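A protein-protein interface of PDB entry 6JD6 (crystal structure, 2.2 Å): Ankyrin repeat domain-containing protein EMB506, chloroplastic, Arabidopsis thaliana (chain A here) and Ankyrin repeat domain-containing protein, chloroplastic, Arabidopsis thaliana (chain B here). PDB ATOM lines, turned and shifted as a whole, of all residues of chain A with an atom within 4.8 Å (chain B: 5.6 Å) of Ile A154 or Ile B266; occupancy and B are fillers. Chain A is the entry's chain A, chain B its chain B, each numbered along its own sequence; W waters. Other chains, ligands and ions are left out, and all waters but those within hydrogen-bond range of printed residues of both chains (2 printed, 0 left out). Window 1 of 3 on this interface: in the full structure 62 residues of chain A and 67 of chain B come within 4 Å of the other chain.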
ATOM      1  N   GLN A 146     -19.498 -18.459  -9.309  1.00  0.00           N
ATOM      2  CA  GLN A 146     -18.736 -17.276  -8.929  1.00  0.00           C
ATOM      3  C   GLN A 146     -19.204 -16.733  -7.587  1.00  0.00           C
ATOM      4  O   GLN A 146     -20.400 -16.724  -7.291  1.00  0.00           O
ATOM      5  CB  GLN A 146     -18.860 -16.180  -9.989  1.00  0.00           C
ATOM      6  CG  GLN A 146     -18.194 -16.511 -11.319  1.00  0.00           C
ATOM      7  CD  GLN A 146     -18.196 -15.332 -12.278  1.00  0.00           C
ATOM      8  OE1 GLN A 146     -19.057 -14.455 -12.201  1.00  0.00           O
ATOM      9  NE2 GLN A 146     -17.226 -15.303 -13.182  1.00  0.00           N
ATOM     10  N   HIS A 150     -15.058 -12.995  -6.873  1.00  0.00           N
ATOM     11  CA  HIS A 150     -14.884 -13.091  -8.323  1.00  0.00           C
ATOM     12  C   HIS A 150     -15.456 -11.855  -9.011  1.00  0.00           C
ATOM     13  O   HIS A 150     -14.791 -11.223  -9.829  1.00  0.00           O
ATOM     14  CB  HIS A 150     -15.609 -14.315  -8.885  1.00  0.00           C
ATOM     15  CG  HIS A 150     -14.908 -15.617  -8.644  1.00  0.00           C
ATOM     16  ND1 HIS A 150     -15.412 -16.587  -7.805  1.00  0.00           N
ATOM     17  CD2 HIS A 150     -13.766 -16.127  -9.165  1.00  0.00           C
ATOM     18  CE1 HIS A 150     -14.602 -17.632  -7.805  1.00  0.00           C
ATOM     19  NE2 HIS A 150     -13.596 -17.379  -8.623  1.00  0.00           N
ATOM     20  N   LYS A 151     -16.696 -11.518  -8.667  1.00  0.00           N
ATOM     21  CA  LYS A 151     -17.393 -10.407  -9.308  1.00  0.00           C
ATOM     22  C   LYS A 151     -16.767  -9.063  -8.995  1.00  0.00           C
ATOM     23  O   LYS A 151     -16.648  -8.206  -9.875  1.00  0.00           O
ATOM     24  CB  LYS A 151     -18.867 -10.391  -8.914  1.00  0.00           C
ATOM     25  CG  LYS A 151     -19.756 -10.947  -9.982  1.00  0.00           C
ATOM     26  CD  LYS A 151     -19.607 -10.170 -11.276  1.00  0.00           C
ATOM     27  CE  LYS A 151     -20.145 -10.985 -12.428  1.00  0.00           C
ATOM     28  NZ  LYS A 151     -21.533 -11.425 -12.140  1.00  0.00           N
ATOM     29  N   ALA A 152     -16.375  -8.881  -7.739  1.00  0.00           N
ATOM     30  CA  ALA A 152     -15.734  -7.645  -7.311  1.00  0.00           C
ATOM     31  C   ALA A 152     -14.439  -7.412  -8.081  1.00  0.00           C
ATOM     32  O   ALA A 152     -14.061  -6.272  -8.360  1.00  0.00           O
ATOM     33  CB  ALA A 152     -15.460  -7.687  -5.814  1.00  0.00           C
ATOM     34  N   ILE A 153     -13.756  -8.503  -8.412  1.00  0.00           N
ATOM     35  CA  ILE A 153     -12.508  -8.421  -9.162  1.00  0.00           C
ATOM     36  C   ILE A 153     -12.790  -8.135 -10.633  1.00  0.00           C
ATOM     37  O   ILE A 153     -12.145  -7.286 -11.240  1.00  0.00           O
ATOM     38  CB  ILE A 153     -11.678  -9.707  -8.996  1.00  0.00           C
ATOM     39  CG1 ILE A 153     -11.184  -9.813  -7.550  1.00  0.00           C
ATOM     40  CG2 ILE A 153     -10.505  -9.715  -9.947  1.00  0.00           C
ATOM     41  CD1 ILE A 153     -10.477 -11.104  -7.237  1.00  0.00           C
ATOM     42  N   ILE A 154     -13.771  -8.837 -11.192  1.00  0.00           N
ATOM     43  CA  ILE A 154     -14.226  -8.598 -12.558  1.00  0.00           C
ATOM     44  C   ILE A 154     -14.651  -7.136 -12.755  1.00  0.00           C
ATOM     45  O   ILE A 154     -14.497  -6.573 -13.842  1.00  0.00           O
ATOM     46  CB  ILE A 154     -15.378  -9.557 -12.919  1.00  0.00           C
ATOM     47  CG1 ILE A 154     -14.861 -10.997 -12.998  1.00  0.00           C
ATOM     48  CG2 ILE A 154     -16.046  -9.163 -14.236  1.00  0.00           C
ATOM     49  CD1 ILE A 154     -15.959 -12.034 -13.141  1.00  0.00           C
ATOM     50  N   GLY A 155     -15.159  -6.518 -11.691  1.00  0.00           N
ATOM     51  CA  GLY A 155     -15.547  -5.118 -11.728  1.00  0.00           C
ATOM     52  C   GLY A 155     -14.420  -4.198 -11.299  1.00  0.00           C
ATOM     53  O   GLY A 155     -14.565  -2.976 -11.318  1.00  0.00           O
ATOM     54  N   LYS A 156     -13.288  -4.787 -10.917  1.00  0.00           N
ATOM     55  CA  LYS A 156     -12.126  -4.023 -10.453  1.00  0.00           C
ATOM     56  C   LYS A 156     -12.496  -3.040  -9.332  1.00  0.00           C
ATOM     57  O   LYS A 156     -12.105  -1.871  -9.342  1.00  0.00           O
ATOM     58  CB  LYS A 156     -11.438  -3.313 -11.628  1.00  0.00           C
ATOM     59  CG  LYS A 156      -9.995  -2.880 -11.353  1.00  0.00           C
ATOM     60  CD  LYS A 156      -9.324  -2.369 -12.619  1.00  0.00           C
ATOM     61  CE  LYS A 156      -7.938  -1.814 -12.335  1.00  0.00           C
ATOM     62  NZ  LYS A 156      -8.001  -0.607 -11.471  1.00  0.00           N
ATOM     63  N   LYS A 157     -13.264  -3.534  -8.368  1.00  0.00           N
ATOM     64  CA  LYS A 157     -13.660  -2.757  -7.199  1.00  0.00           C
ATOM     65  C   LYS A 157     -12.688  -3.038  -6.059  1.00  0.00           C
ATOM     66  O   LYS A 157     -12.987  -3.813  -5.148  1.00  0.00           O
ATOM     67  CB  LYS A 157     -15.083  -3.143  -6.786  1.00  0.00           C
ATOM     68  CG  LYS A 157     -16.161  -2.161  -7.225  1.00  0.00           C
ATOM     69  CD  LYS A 157     -16.403  -2.117  -8.723  1.00  0.00           C
ATOM     70  CE  LYS A 157     -17.203  -0.855  -9.063  1.00  0.00           C
ATOM     71  NZ  LYS A 157     -18.063  -0.938 -10.284  1.00  0.00           N
ATOM     72  N   TYR A 184      -8.890 -13.343 -13.090  1.00  0.00           N
ATOM     73  CA  TYR A 184      -9.661 -12.135 -13.367  1.00  0.00           C
ATOM     74  C   TYR A 184      -8.919 -10.855 -12.990  1.00  0.00           C
ATOM     75  O   TYR A 184      -9.071  -9.832 -13.653  1.00  0.00           O
ATOM     76  CB  TYR A 184     -11.025 -12.190 -12.670  1.00  0.00           C
ATOM     77  CG  TYR A 184     -11.961 -13.239 -13.230  1.00  0.00           C
ATOM     78  CD1 TYR A 184     -12.394 -13.179 -14.546  1.00  0.00           C
ATOM     79  CD2 TYR A 184     -12.433 -14.274 -12.432  1.00  0.00           C
ATOM     80  CE1 TYR A 184     -13.261 -14.132 -15.057  1.00  0.00           C
ATOM     81  CE2 TYR A 184     -13.294 -15.231 -12.934  1.00  0.00           C
ATOM     82  CZ  TYR A 184     -13.704 -15.154 -14.246  1.00  0.00           C
ATOM     83  OH  TYR A 184     -14.568 -16.106 -14.746  1.00  0.00           O
ATOM     84  N   VAL A 188      -8.325  -7.849 -15.825  1.00  0.00           N
ATOM     85  CA  VAL A 188      -8.734  -6.448 -15.708  1.00  0.00           C
ATOM     86  C   VAL A 188      -7.551  -5.538 -15.390  1.00  0.00           C
ATOM     87  O   VAL A 188      -7.722  -4.342 -15.159  1.00  0.00           O
ATOM     88  CB  VAL A 188      -9.882  -6.246 -14.675  1.00  0.00           C
ATOM     89  CG1 VAL A 188     -11.061  -7.152 -15.014  1.00  0.00           C
ATOM     90  CG2 VAL A 188      -9.396  -6.512 -13.255  1.00  0.00           C
ATOM     91  N   LEU B 258     -21.047 -13.062 -23.392  1.00  0.00           N
ATOM     92  CA  LEU B 258     -20.813 -11.630 -23.225  1.00  0.00           C
ATOM     93  C   LEU B 258     -19.969 -11.080 -24.371  1.00  0.00           C
ATOM     94  O   LEU B 258     -19.162 -11.800 -24.952  1.00  0.00           O
ATOM     95  CB  LEU B 258     -20.106 -11.348 -21.899  1.00  0.00           C
ATOM     96  CG  LEU B 258     -20.803 -11.777 -20.607  1.00  0.00           C
ATOM     97  CD1 LEU B 258     -19.968 -11.337 -19.415  1.00  0.00           C
ATOM     98  CD2 LEU B 258     -22.213 -11.205 -20.525  1.00  0.00           C
ATOM     99  N   LEU B 261     -18.516  -5.052 -25.114  1.00  0.00           N
ATOM    100  CA  LEU B 261     -19.286  -3.983 -24.472  1.00  0.00           C
ATOM    101  C   LEU B 261     -19.600  -4.308 -23.020  1.00  0.00           C
ATOM    102  O   LEU B 261     -19.493  -3.441 -22.156  1.00  0.00           O
ATOM    103  CB  LEU B 261     -20.583  -3.705 -25.236  1.00  0.00           C
ATOM    104  CG  LEU B 261     -20.533  -2.537 -26.223  1.00  0.00           C
ATOM    105  CD1 LEU B 261     -21.847  -2.422 -26.987  1.00  0.00           C
ATOM    106  CD2 LEU B 261     -20.222  -1.235 -25.493  1.00  0.00           C
ATOM    107  N   HIS B 262     -19.984  -5.553 -22.754  1.00  0.00           N
ATOM    108  CA  HIS B 262     -20.201  -6.005 -21.383  1.00  0.00           C
ATOM    109  C   HIS B 262     -18.963  -5.769 -20.533  1.00  0.00           C
ATOM    110  O   HIS B 262     -19.055  -5.259 -19.418  1.00  0.00           O
ATOM    111  CB  HIS B 262     -20.545  -7.496 -21.340  1.00  0.00           C
ATOM    112  CG  HIS B 262     -21.923  -7.820 -21.827  1.00  0.00           C
ATOM    113  ND1 HIS B 262     -22.162  -8.410 -23.050  1.00  0.00           N
ATOM    114  CD2 HIS B 262     -23.136  -7.645 -21.249  1.00  0.00           C
ATOM    115  CE1 HIS B 262     -23.462  -8.582 -23.207  1.00  0.00           C
ATOM    116  NE2 HIS B 262     -24.077  -8.123 -22.130  1.00  0.00           N
ATOM    117  N   ARG B 263     -17.806  -6.151 -21.064  1.00  0.00           N
ATOM    118  CA  ARG B 263     -16.555  -6.057 -20.320  1.00  0.00           C
ATOM    119  C   ARG B 263     -16.158  -4.603 -20.057  1.00  0.00           C
ATOM    120  O   ARG B 263     -15.739  -4.257 -18.954  1.00  0.00           O
ATOM    121  CB  ARG B 263     -15.435  -6.807 -21.055  1.00  0.00           C
ATOM    122  CG  ARG B 263     -15.724  -8.296 -21.276  1.00  0.00           C
ATOM    123  CD  ARG B 263     -16.216  -8.981 -19.991  1.00  0.00           C
ATOM    124  NE  ARG B 263     -15.299  -8.780 -18.868  1.00  0.00           N
ATOM    125  CZ  ARG B 263     -14.307  -9.611 -18.559  1.00  0.00           C
ATOM    126  NH1 ARG B 263     -14.104 -10.703 -19.287  1.00  0.00           N
ATOM    127  NH2 ARG B 263     -13.518  -9.353 -17.521  1.00  0.00           N
ATOM    128  N   ALA B 264     -16.296  -3.754 -21.068  1.00  0.00           N
ATOM    129  CA  ALA B 264     -15.991  -2.338 -20.910  1.00  0.00           C
ATOM    130  C   ALA B 264     -16.930  -1.686 -19.890  1.00  0.00           C
ATOM    131  O   ALA B 264     -16.513  -0.854 -19.079  1.00  0.00           O
ATOM    132  CB  ALA B 264     -16.081  -1.627 -22.254  1.00  0.00           C
ATOM    133  N   ILE B 265     -18.198  -2.083 -19.922  1.00  0.00           N
ATOM    134  CA  ILE B 265     -19.197  -1.506 -19.027  1.00  0.00           C
ATOM    135  C   ILE B 265     -19.022  -1.958 -17.576  1.00  0.00           C
ATOM    136  O   ILE B 265     -19.017  -1.132 -16.661  1.00  0.00           O
ATOM    137  CB  ILE B 265     -20.624  -1.801 -19.519  1.00  0.00           C
ATOM    138  CG1 ILE B 265     -20.923  -0.957 -20.762  1.00  0.00           C
ATOM    139  CG2 ILE B 265     -21.646  -1.519 -18.421  1.00  0.00           C
ATOM    140  CD1 ILE B 265     -22.245  -1.258 -21.411  1.00  0.00           C
ATOM    141  N   ILE B 266     -18.869  -3.264 -17.370  1.00  0.00           N
ATOM    142  CA  ILE B 266     -18.712  -3.821 -16.027  1.00  0.00           C
ATOM    143  C   ILE B 266     -17.504  -3.213 -15.305  1.00  0.00           C
ATOM    144  O   ILE B 266     -17.564  -2.925 -14.106  1.00  0.00           O
ATOM    145  CB  ILE B 266     -18.592  -5.365 -16.065  1.00  0.00           C
ATOM    146  CG1 ILE B 266     -19.895  -5.988 -16.566  1.00  0.00           C
ATOM    147  CG2 ILE B 266     -18.278  -5.922 -14.689  1.00  0.00           C
ATOM    148  CD1 ILE B 266     -19.752  -7.441 -16.971  1.00  0.00           C
ATOM    149  N   GLY B 267     -16.416  -3.001 -16.042  1.00  0.00           N
ATOM    150  CA  GLY B 267     -15.219  -2.416 -15.467  1.00  0.00           C
ATOM    151  C   GLY B 267     -15.215  -0.897 -15.468  1.00  0.00           C
ATOM    152  O   GLY B 267     -14.221  -0.277 -15.092  1.00  0.00           O
ATOM    153  N   LYS B 268     -16.328  -0.301 -15.888  1.00  0.00           N
ATOM    154  CA  LYS B 268     -16.453   1.154 -15.975  1.00  0.00           C
ATOM    155  C   LYS B 268     -15.339   1.791 -16.807  1.00  0.00           C
ATOM    156  O   LYS B 268     -14.799   2.836 -16.449  1.00  0.00           O
ATOM    157  CB  LYS B 268     -16.535   1.793 -14.580  1.00  0.00           C
ATOM    158  CG  LYS B 268     -17.818   1.453 -13.832  1.00  0.00           C
ATOM    159  CD  LYS B 268     -17.804   1.980 -12.399  1.00  0.00           C
ATOM    160  CE  LYS B 268     -18.557   3.284 -12.272  1.00  0.00           C
ATOM    161  NZ  LYS B 268     -18.796   3.628 -10.840  1.00  0.00           N
ATOM    162  N   TYR B 296     -26.469  -4.082 -16.675  1.00  0.00           N
ATOM    163  CA  TYR B 296     -25.065  -4.097 -16.275  1.00  0.00           C
ATOM    164  C   TYR B 296     -24.562  -2.716 -15.875  1.00  0.00           C
ATOM    165  O   TYR B 296     -23.814  -2.575 -14.903  1.00  0.00           O
ATOM    166  CB  TYR B 296     -24.199  -4.659 -17.402  1.00  0.00           C
ATOM    167  CG  TYR B 296     -24.284  -6.161 -17.518  1.00  0.00           C
ATOM    168  CD1 TYR B 296     -23.381  -6.977 -16.847  1.00  0.00           C
ATOM    169  CD2 TYR B 296     -25.274  -6.765 -18.282  1.00  0.00           C
ATOM    170  CE1 TYR B 296     -23.456  -8.356 -16.944  1.00  0.00           C
ATOM    171  CE2 TYR B 296     -25.362  -8.139 -18.381  1.00  0.00           C
ATOM    172  CZ  TYR B 296     -24.447  -8.929 -17.714  1.00  0.00           C
ATOM    173  OH  TYR B 296     -24.526 -10.299 -17.811  1.00  0.00           O
ATOM    174  N   THR B 300     -23.288  -1.864 -11.882  1.00  0.00           N
ATOM    175  CA  THR B 300     -21.960  -1.348 -11.611  1.00  0.00           C
ATOM    176  C   THR B 300     -22.024   0.132 -11.228  1.00  0.00           C
ATOM    177  O   THR B 300     -20.997   0.778 -11.012  1.00  0.00           O
ATOM    178  CB  THR B 300     -21.031  -1.588 -12.826  1.00  0.00           C
ATOM    179  OG1 THR B 300     -19.667  -1.638 -12.390  1.00  0.00           O
ATOM    180  CG2 THR B 300     -21.222  -0.501 -13.891  1.00  0.00           C
HETATM  181  O   HOH W   1     -19.409   1.561  -8.674  1.00  0.00           O
HETATM  182  O   HOH W   2     -14.397  -6.585 -17.023  1.00  0.00           O
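The backbone NH of Lys A157 sits at hydrogen-bond distance from the backbone carbonyl oxygen of Ala A152 (2.9 Å). The backbone carbonyl oxygen (O) of Ile B266 is in hydrogen-bond range of the side-chain hydroxyl (OG1) of Thr B300 (3.0 Å).
Hydrophobic or aromatic side chains of chain A within 4 Å of the printed part of chain B: Ile A154. Of the 11 printed residues of chain B, 3 touch a printed residue of chain A. Among the printed residues, 4 pairs touch across the chains.
Water W1 lies within hydrogen-bond range of O of Thr B300 (2.9 Å), NZ of Lys B268 (3.1 Å) and NZ of Lys A157 (3.3 Å). Water W2 bridges the guanidinium group of Arg B263 and the backbone carbonyl oxygen of Ile A154.
NZ of Lys A157 sits at hydrogen-bond distance from OG1 of Thr B300 (2.7 Å).
Of chain B, only Ile B266 (3.9 Å) comes within 4 Å of Ile A154. Ile B266 touches just these residues of chain A: Ile A154 and Gly A155. Printed residues of chain A within 4 Å of Thr B300: Lys A157. Of the printed residues of chain B, Gly A155 touches Ile B266 (3.8 Å). Of the printed residues of chain B, Lys A157 touches Lys B268 (3.6 Å) and Thr B300 (2.7 Å). The nearest residue of chain B that does not touch Ile A154 is Arg B263 (4.1 Å). The nearest residue of chain A that does not touch Ile B266 is Lys A157 (4.3 Å).
Among the printed residues, pairs that only touch across the chains: Ile A154 with Ile B266, Gly A155 with Ile B266 and Lys A157 with Lys B268.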
